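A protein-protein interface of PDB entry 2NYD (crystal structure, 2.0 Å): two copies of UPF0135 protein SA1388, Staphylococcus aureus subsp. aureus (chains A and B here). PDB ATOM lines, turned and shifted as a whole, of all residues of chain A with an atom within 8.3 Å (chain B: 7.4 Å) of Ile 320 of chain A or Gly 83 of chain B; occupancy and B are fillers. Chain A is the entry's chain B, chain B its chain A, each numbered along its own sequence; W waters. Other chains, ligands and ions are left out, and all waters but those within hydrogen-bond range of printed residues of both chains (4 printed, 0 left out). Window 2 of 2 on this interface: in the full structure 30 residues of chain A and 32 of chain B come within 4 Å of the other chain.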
ATOM      1  N   VAL A 273     -29.422 -25.225 -32.188  1.00  0.00           N
ATOM      2  CA  VAL A 273     -29.670 -24.103 -31.311  1.00  0.00           C
ATOM      3  C   VAL A 273     -29.920 -22.938 -32.223  1.00  0.00           C
ATOM      4  O   VAL A 273     -29.065 -22.586 -33.041  1.00  0.00           O
ATOM      5  CB  VAL A 273     -28.471 -23.792 -30.363  1.00  0.00           C
ATOM      6  CG1 VAL A 273     -28.763 -22.542 -29.452  1.00  0.00           C
ATOM      7  CG2 VAL A 273     -28.180 -24.999 -29.486  1.00  0.00           C
ATOM      8  N   GLY A 274     -31.097 -22.341 -32.075  1.00  0.00           N
ATOM      9  CA  GLY A 274     -31.474 -21.179 -32.900  1.00  0.00           C
ATOM     10  C   GLY A 274     -32.934 -21.269 -33.303  1.00  0.00           C
ATOM     11  O   GLY A 274     -33.559 -22.322 -33.118  1.00  0.00           O
ATOM     12  N   TYR A 295     -18.138 -18.317 -31.838  1.00  0.00           N
ATOM     13  CA  TYR A 295     -18.202 -16.850 -31.885  1.00  0.00           C
ATOM     14  C   TYR A 295     -17.315 -16.292 -33.007  1.00  0.00           C
ATOM     15  O   TYR A 295     -17.729 -15.391 -33.741  1.00  0.00           O
ATOM     16  CB  TYR A 295     -17.900 -16.260 -30.518  1.00  0.00           C
ATOM     17  CG  TYR A 295     -18.921 -16.701 -29.498  1.00  0.00           C
ATOM     18  CD1 TYR A 295     -18.676 -17.785 -28.660  1.00  0.00           C
ATOM     19  CD2 TYR A 295     -20.167 -16.038 -29.396  1.00  0.00           C
ATOM     20  CE1 TYR A 295     -19.655 -18.191 -27.704  1.00  0.00           C
ATOM     21  CE2 TYR A 295     -21.142 -16.441 -28.480  1.00  0.00           C
ATOM     22  CZ  TYR A 295     -20.880 -17.528 -27.658  1.00  0.00           C
ATOM     23  OH  TYR A 295     -21.828 -17.923 -26.786  1.00  0.00           O
ATOM     24  N   HIS A 313     -24.613 -25.580 -21.231  1.00  0.00           N
ATOM     25  CA  HIS A 313     -24.340 -24.174 -20.906  1.00  0.00           C
ATOM     26  C   HIS A 313     -23.745 -23.462 -22.096  1.00  0.00           C
ATOM     27  O   HIS A 313     -24.011 -22.279 -22.314  1.00  0.00           O
ATOM     28  CB  HIS A 313     -23.436 -24.067 -19.684  1.00  0.00           C
ATOM     29  CG  HIS A 313     -24.174 -24.234 -18.400  1.00  0.00           C
ATOM     30  ND1 HIS A 313     -25.089 -23.303 -17.946  1.00  0.00           N
ATOM     31  CD2 HIS A 313     -24.206 -25.262 -17.523  1.00  0.00           C
ATOM     32  CE1 HIS A 313     -25.617 -23.741 -16.815  1.00  0.00           C
ATOM     33  NE2 HIS A 313     -25.089 -24.922 -16.533  1.00  0.00           N
ATOM     34  N   ASP A 314     -22.955 -24.176 -22.901  1.00  0.00           N
ATOM     35  CA  ASP A 314     -22.473 -23.524 -24.136  1.00  0.00           C
ATOM     36  C   ASP A 314     -23.553 -23.273 -25.187  1.00  0.00           C
ATOM     37  O   ASP A 314     -23.494 -22.284 -25.927  1.00  0.00           O
ATOM     38  CB  ASP A 314     -21.318 -24.310 -24.767  1.00  0.00           C
ATOM     39  CG  ASP A 314     -20.092 -24.335 -23.853  1.00  0.00           C
ATOM     40  OD1 ASP A 314     -19.679 -23.274 -23.303  1.00  0.00           O
ATOM     41  OD2 ASP A 314     -19.593 -25.438 -23.681  1.00  0.00           O
ATOM     42  N   ALA A 315     -24.492 -24.196 -25.295  1.00  0.00           N
ATOM     43  CA  ALA A 315     -25.683 -23.983 -26.147  1.00  0.00           C
ATOM     44  C   ALA A 315     -26.555 -22.832 -25.603  1.00  0.00           C
ATOM     45  O   ALA A 315     -27.079 -22.019 -26.377  1.00  0.00           O
ATOM     46  CB  ALA A 315     -26.524 -25.299 -26.238  1.00  0.00           C
ATOM     47  N   LEU A 316     -26.741 -22.793 -24.279  1.00  0.00           N
ATOM     48  CA  LEU A 316     -27.508 -21.705 -23.644  1.00  0.00           C
ATOM     49  C   LEU A 316     -26.918 -20.329 -23.978  1.00  0.00           C
ATOM     50  O   LEU A 316     -27.625 -19.445 -24.380  1.00  0.00           O
ATOM     51  CB  LEU A 316     -27.583 -21.902 -22.120  1.00  0.00           C
ATOM     52  CG  LEU A 316     -28.686 -21.085 -21.395  1.00  0.00           C
ATOM     53  CD1 LEU A 316     -30.084 -21.689 -21.623  1.00  0.00           C
ATOM     54  CD2 LEU A 316     -28.381 -21.020 -19.922  1.00  0.00           C
ATOM     55  N   ASP A 317     -25.608 -20.182 -23.775  1.00  0.00           N
ATOM     56  CA  ASP A 317     -24.826 -18.989 -24.167  1.00  0.00           C
ATOM     57  C   ASP A 317     -24.984 -18.653 -25.645  1.00  0.00           C
ATOM     58  O   ASP A 317     -25.302 -17.479 -25.989  1.00  0.00           O
ATOM     59  CB  ASP A 317     -23.330 -19.204 -23.864  1.00  0.00           C
ATOM     60  CG  ASP A 317     -23.036 -19.252 -22.376  1.00  0.00           C
ATOM     61  OD1 ASP A 317     -23.932 -18.982 -21.559  1.00  0.00           O
ATOM     62  OD2 ASP A 317     -21.907 -19.590 -21.999  1.00  0.00           O
ATOM     63  N   ALA A 318     -24.814 -19.657 -26.527  1.00  0.00           N
ATOM     64  CA  ALA A 318     -24.984 -19.430 -27.959  1.00  0.00           C
ATOM     65  C   ALA A 318     -26.387 -18.885 -28.262  1.00  0.00           C
ATOM     66  O   ALA A 318     -26.510 -17.902 -28.996  1.00  0.00           O
ATOM     67  CB  ALA A 318     -24.720 -20.692 -28.780  1.00  0.00           C
ATOM     68  N   LYS A 319     -27.412 -19.521 -27.690  1.00  0.00           N
ATOM     69  CA  LYS A 319     -28.802 -19.105 -27.905  1.00  0.00           C
ATOM     70  C   LYS A 319     -29.031 -17.618 -27.551  1.00  0.00           C
ATOM     71  O   LYS A 319     -29.574 -16.828 -28.379  1.00  0.00           O
ATOM     72  CB  LYS A 319     -29.804 -19.986 -27.137  1.00  0.00           C
ATOM     73  CG  LYS A 319     -31.285 -19.678 -27.523  1.00  0.00           C
ATOM     74  CD  LYS A 319     -32.228 -20.813 -27.180  1.00  0.00           C
ATOM     75  CE  LYS A 319     -33.710 -20.475 -27.513  1.00  0.00           C
ATOM     76  NZ  LYS A 319     -33.951 -20.601 -29.026  1.00  0.00           N
ATOM     77  N   ILE A 320     -28.644 -17.244 -26.338  1.00  0.00           N
ATOM     78  CA  ILE A 320     -28.826 -15.860 -25.897  1.00  0.00           C
ATOM     79  C   ILE A 320     -28.064 -14.854 -26.764  1.00  0.00           C
ATOM     80  O   ILE A 320     -28.482 -13.692 -26.914  1.00  0.00           O
ATOM     81  CB  ILE A 320     -28.550 -15.685 -24.377  1.00  0.00           C
ATOM     82  CG1 ILE A 320     -29.410 -14.519 -23.849  1.00  0.00           C
ATOM     83  CG2 ILE A 320     -27.066 -15.450 -24.078  1.00  0.00           C
ATOM     84  CD1 ILE A 320     -29.324 -14.300 -22.355  1.00  0.00           C
ATOM     85  N   HIS A 321     -26.960 -15.296 -27.382  1.00  0.00           N
ATOM     86  CA  HIS A 321     -26.199 -14.393 -28.224  1.00  0.00           C
ATOM     87  C   HIS A 321     -26.585 -14.442 -29.680  1.00  0.00           C
ATOM     88  O   HIS A 321     -25.980 -13.757 -30.482  1.00  0.00           O
ATOM     89  CB  HIS A 321     -24.691 -14.630 -28.054  1.00  0.00           C
ATOM     90  CG  HIS A 321     -24.186 -14.287 -26.692  1.00  0.00           C
ATOM     91  ND1 HIS A 321     -24.300 -13.020 -26.149  1.00  0.00           N
ATOM     92  CD2 HIS A 321     -23.592 -15.051 -25.747  1.00  0.00           C
ATOM     93  CE1 HIS A 321     -23.801 -13.023 -24.928  1.00  0.00           C
ATOM     94  NE2 HIS A 321     -23.364 -14.245 -24.661  1.00  0.00           N
ATOM     95  N   GLY A 322     -27.584 -15.259 -30.028  1.00  0.00           N
ATOM     96  CA  GLY A 322     -27.972 -15.422 -31.409  1.00  0.00           C
ATOM     97  C   GLY A 322     -26.983 -16.184 -32.257  1.00  0.00           C
ATOM     98  O   GLY A 322     -27.033 -16.091 -33.472  1.00  0.00           O
ATOM     99  N   VAL A 323     -26.064 -16.930 -31.647  1.00  0.00           N
ATOM    100  CA  VAL A 323     -25.142 -17.799 -32.416  1.00  0.00           C
ATOM    101  C   VAL A 323     -25.841 -19.161 -32.690  1.00  0.00           C
ATOM    102  O   VAL A 323     -26.223 -19.893 -31.751  1.00  0.00           O
ATOM    103  CB  VAL A 323     -23.771 -17.991 -31.686  1.00  0.00           C
ATOM    104  CG1 VAL A 323     -22.856 -19.042 -32.477  1.00  0.00           C
ATOM    105  CG2 VAL A 323     -23.033 -16.670 -31.547  1.00  0.00           C
ATOM    106  N   CYS B  49     -32.849 -19.075 -15.516  1.00  0.00           N
ATOM    107  CA  CYS B  49     -33.614 -17.844 -15.503  1.00  0.00           C
ATOM    108  C   CYS B  49     -33.395 -17.131 -16.819  1.00  0.00           C
ATOM    109  O   CYS B  49     -32.509 -16.319 -16.922  1.00  0.00           O
ATOM    110  CB  CYS B  49     -33.217 -16.964 -14.296  1.00  0.00           C
ATOM    111  SG  CYS B  49     -34.286 -15.443 -14.202  1.00  0.00           S
ATOM    112  N   THR B  50     -34.200 -17.469 -17.834  1.00  0.00           N
ATOM    113  CA  THR B  50     -34.107 -16.831 -19.128  1.00  0.00           C
ATOM    114  C   THR B  50     -34.969 -15.546 -19.114  1.00  0.00           C
ATOM    115  O   THR B  50     -35.740 -15.293 -18.172  1.00  0.00           O
ATOM    116  CB  THR B  50     -34.621 -17.743 -20.243  1.00  0.00           C
ATOM    117  OG1 THR B  50     -36.027 -17.930 -20.059  1.00  0.00           O
ATOM    118  CG2 THR B  50     -33.831 -19.150 -20.259  1.00  0.00           C
ATOM    119  N   LEU B  51     -34.839 -14.750 -20.157  1.00  0.00           N
ATOM    120  CA  LEU B  51     -35.678 -13.576 -20.317  1.00  0.00           C
ATOM    121  C   LEU B  51     -37.173 -13.945 -20.324  1.00  0.00           C
ATOM    122  O   LEU B  51     -38.003 -13.213 -19.774  1.00  0.00           O
ATOM    123  CB  LEU B  51     -35.324 -12.836 -21.616  1.00  0.00           C
ATOM    124  CG  LEU B  51     -35.965 -11.428 -21.754  1.00  0.00           C
ATOM    125  CD1 LEU B  51     -35.544 -10.489 -20.629  1.00  0.00           C
ATOM    126  CD2 LEU B  51     -35.660 -10.779 -23.125  1.00  0.00           C
ATOM    127  N   LEU B  71     -27.654 -17.341 -12.503  1.00  0.00           N
ATOM    128  CA  LEU B  71     -27.638 -16.476 -13.676  1.00  0.00           C
ATOM    129  C   LEU B  71     -26.303 -15.716 -13.751  1.00  0.00           C
ATOM    130  O   LEU B  71     -25.842 -15.384 -14.823  1.00  0.00           O
ATOM    131  CB  LEU B  71     -28.805 -15.464 -13.647  1.00  0.00           C
ATOM    132  CG  LEU B  71     -28.911 -14.377 -14.718  1.00  0.00           C
ATOM    133  CD1 LEU B  71     -29.084 -15.000 -16.104  1.00  0.00           C
ATOM    134  CD2 LEU B  71     -30.072 -13.436 -14.399  1.00  0.00           C
ATOM    135  N   LYS B  80     -25.056  -4.484 -19.880  1.00  0.00           N
ATOM    136  CA  LYS B  80     -25.593  -3.790 -21.020  1.00  0.00           C
ATOM    137  C   LYS B  80     -26.904  -4.406 -21.483  1.00  0.00           C
ATOM    138  O   LYS B  80     -27.284  -5.509 -21.061  1.00  0.00           O
ATOM    139  CB  LYS B  80     -24.531  -3.765 -22.135  1.00  0.00           C
ATOM    140  CG  LYS B  80     -23.248  -2.992 -21.683  1.00  0.00           C
ATOM    141  CD  LYS B  80     -22.168  -2.955 -22.755  1.00  0.00           C
ATOM    142  CE  LYS B  80     -21.669  -4.357 -23.127  1.00  0.00           C
ATOM    143  NZ  LYS B  80     -20.679  -4.233 -24.266  1.00  0.00           N
ATOM    144  N   ALA B  81     -27.607  -3.711 -22.361  1.00  0.00           N
ATOM    145  CA  ALA B  81     -28.897  -4.188 -22.844  1.00  0.00           C
ATOM    146  C   ALA B  81     -28.697  -5.207 -23.956  1.00  0.00           C
ATOM    147  O   ALA B  81     -29.135  -5.037 -25.084  1.00  0.00           O
ATOM    148  CB  ALA B  81     -29.765  -3.007 -23.287  1.00  0.00           C
ATOM    149  N   ASN B  82     -28.028  -6.304 -23.633  1.00  0.00           N
ATOM    150  CA  ASN B  82     -27.713  -7.309 -24.635  1.00  0.00           C
ATOM    151  C   ASN B  82     -27.362  -8.618 -23.903  1.00  0.00           C
ATOM    152  O   ASN B  82     -26.808  -8.575 -22.828  1.00  0.00           O
ATOM    153  CB  ASN B  82     -26.484  -6.814 -25.411  1.00  0.00           C
ATOM    154  CG  ASN B  82     -26.004  -7.799 -26.390  1.00  0.00           C
ATOM    155  OD1 ASN B  82     -26.615  -7.964 -27.454  1.00  0.00           O
ATOM    156  ND2 ASN B  82     -24.925  -8.528 -26.035  1.00  0.00           N
ATOM    157  N   GLY B  83     -27.695  -9.785 -24.463  1.00  0.00           N
ATOM    158  CA  GLY B  83     -27.212 -11.051 -23.873  1.00  0.00           C
ATOM    159  C   GLY B  83     -27.786 -11.240 -22.481  1.00  0.00           C
ATOM    160  O   GLY B  83     -28.945 -10.892 -22.210  1.00  0.00           O
ATOM    161  N   TYR B  84     -26.968 -11.769 -21.591  1.00  0.00           N
ATOM    162  CA  TYR B  84     -27.353 -11.951 -20.198  1.00  0.00           C
ATOM    163  C   TYR B  84     -27.609 -10.585 -19.508  1.00  0.00           C
ATOM    164  O   TYR B  84     -28.369 -10.513 -18.566  1.00  0.00           O
ATOM    165  CB  TYR B  84     -26.285 -12.762 -19.428  1.00  0.00           C
ATOM    166  CG  TYR B  84     -26.249 -14.229 -19.821  1.00  0.00           C
ATOM    167  CD1 TYR B  84     -25.197 -14.739 -20.593  1.00  0.00           C
ATOM    168  CD2 TYR B  84     -27.282 -15.097 -19.436  1.00  0.00           C
ATOM    169  CE1 TYR B  84     -25.171 -16.095 -20.988  1.00  0.00           C
ATOM    170  CE2 TYR B  84     -27.274 -16.457 -19.799  1.00  0.00           C
ATOM    171  CZ  TYR B  84     -26.202 -16.938 -20.583  1.00  0.00           C
ATOM    172  OH  TYR B  84     -26.183 -18.241 -20.926  1.00  0.00           O
ATOM    173  N   GLY B  85     -26.979  -9.515 -20.021  1.00  0.00           N
ATOM    174  CA  GLY B  85     -27.173  -8.160 -19.475  1.00  0.00           C
ATOM    175  C   GLY B  85     -28.661  -7.799 -19.453  1.00  0.00           C
ATOM    176  O   GLY B  85     -29.141  -7.123 -18.534  1.00  0.00           O
ATOM    177  N   LEU B  86     -29.382  -8.277 -20.465  1.00  0.00           N
ATOM    178  CA  LEU B  86     -30.773  -7.965 -20.705  1.00  0.00           C
ATOM    179  C   LEU B  86     -31.627  -8.574 -19.617  1.00  0.00           C
ATOM    180  O   LEU B  86     -32.545  -7.934 -19.072  1.00  0.00           O
ATOM    181  CB  LEU B  86     -31.152  -8.598 -22.047  1.00  0.00           C
ATOM    182  CG  LEU B  86     -32.002  -7.971 -23.142  1.00  0.00           C
ATOM    183  CD1 LEU B  86     -31.835  -6.486 -23.274  1.00  0.00           C
ATOM    184  CD2 LEU B  86     -31.613  -8.716 -24.481  1.00  0.00           C
ATOM    185  N   ILE B  87     -31.316  -9.811 -19.248  1.00  0.00           N
ATOM    186  CA  ILE B  87     -32.090 -10.475 -18.235  1.00  0.00           C
ATOM    187  C   ILE B  87     -31.836  -9.844 -16.845  1.00  0.00           C
ATOM    188  O   ILE B  87     -32.769  -9.586 -16.057  1.00  0.00           O
ATOM    189  CB  ILE B  87     -31.716 -11.981 -18.205  1.00  0.00           C
ATOM    190  CG1 ILE B  87     -31.859 -12.613 -19.617  1.00  0.00           C
ATOM    191  CG2 ILE B  87     -32.467 -12.685 -17.072  1.00  0.00           C
ATOM    192  CD1 ILE B  87     -31.313 -14.046 -19.655  1.00  0.00           C
ATOM    193  N   ILE B  88     -30.561  -9.622 -16.535  1.00  0.00           N
ATOM    194  CA  ILE B  88     -30.172  -9.028 -15.238  1.00  0.00           C
ATOM    195  C   ILE B  88     -30.799  -7.633 -15.074  1.00  0.00           C
ATOM    196  O   ILE B  88     -31.387  -7.300 -14.015  1.00  0.00           O
ATOM    197  CB  ILE B  88     -28.623  -8.902 -15.156  1.00  0.00           C
ATOM    198  CG1 ILE B  88     -27.962 -10.302 -15.095  1.00  0.00           C
ATOM    199  CG2 ILE B  88     -28.211  -8.081 -13.860  1.00  0.00           C
ATOM    200  CD1 ILE B  88     -26.493 -10.387 -15.613  1.00  0.00           C
ATOM    201  N   PRO B 366     -32.001 -24.846 -24.657  1.00  0.00           N
ATOM    202  CA  PRO B 366     -31.500 -24.230 -25.905  1.00  0.00           C
ATOM    203  C   PRO B 366     -31.504 -25.194 -27.118  1.00  0.00           C
ATOM    204  O   PRO B 366     -31.454 -24.734 -28.225  1.00  0.00           O
ATOM    205  CB  PRO B 366     -30.072 -23.805 -25.537  1.00  0.00           C
ATOM    206  CG  PRO B 366     -29.659 -24.808 -24.444  1.00  0.00           C
ATOM    207  CD  PRO B 366     -30.955 -24.925 -23.621  1.00  0.00           C
HETATM  208  O   HOH W   1     -34.645 -23.688 -27.605  1.00  0.00           O
HETATM  209  O   HOH W   2     -25.404 -10.710 -27.361  1.00  0.00           O
HETATM  210  O   HOH W   3     -32.843 -23.280 -29.875  1.00  0.00           O
HETATM  211  O   HOH W   4     -24.732 -20.784 -19.242  1.00  0.00           O
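Of chain B, only Gly 83 (3.4 Å), Tyr 84 (3.5 Å) and Ile 87 (3.4 Å) come within 4 Å of Ile 320 of chain A. Of chain A, only Ile 320 comes within 4 Å of Gly 83 of chain B. Of the printed residues of chain B, Lys 319 of chain A touches Pro 366 (3.7 Å). Printed residues of chain B within 4 Å of Ala 315 of chain A: Pro 366 (3.6 Å). Of the printed residues of chain B, Leu 316 of chain A touches Tyr 84 (3.7 Å) and Pro 366 (3.5 Å). Leu 86 of chain B touches none of the printed residues of chain A. Thr 50 of chain B touches none of the printed residues of chain A. The nearest residue of chain B that does not touch Ile 320 of chain A is Gly 85 of chain B (5.8 Å). The nearest residue of chain A that does not touch Gly 83 of chain B is His 321 of chain A (4.1 Å).
Water W2 bridges ND2 of Asn 82 of chain B (2.6 Å) and ND1 of His 321 of chain A (2.8 Å). Water W3 lies within hydrogen-bond range of O of Pro 366 of chain B (2.6 Å), N of Gly 274 of chain A (3.0 Å) and NZ of Lys 319 of chain A (3.0 Å). Water W4 lies within hydrogen-bond range of ND1 of His 313 of chain A, OD1 of Asp 317 of chain A and OH of Tyr 84 of chain B. Water W1 bridges O of Pro 366 of chain B (3.4 Å) and NZ of Lys 319 of chain A (3.5 Å).
OH of Tyr 84 of chain B sits at hydrogen-bond distance from OD1 of Asp 317 of chain A.
Printed residues of chain B that touch a printed residue of chain A: Gly 83, Tyr 84, Ile 87 and Pro 366. Hydrophobic or aromatic side chains of chain B within 4 Å of the printed part of chain A: Tyr 84, Ile 87 and Pro 366. Among the printed residues, 9 pairs touch across the chains. Among the printed residues, no Asp or Glu carboxylate lies within 4 Å of a Lys or Arg side-chain nitrogen of the other chain.
No position is printed for both chains.
Among the printed residues, merely in contact across the chains: Ile 320 of chain A with Ile 87 of chain B (3.4 Å), Ile 320 of chain A with Gly 83 of chain B (3.4 Å), Val 273 of chain A with Pro 366 of chain B (3.5 Å), Ile 320 of chain A with Tyr 84 of chain B (3.5 Å), Leu 316 of chain A with Pro 366 of chain B (3.5 Å), Ala 315 of chain A with Pro 366 of chain B (3.6 Å), Leu 316 of chain A with Tyr 84 of chain B (3.7 Å) and Lys 319 of chain A with Pro 366 of chain B (3.7 Å).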
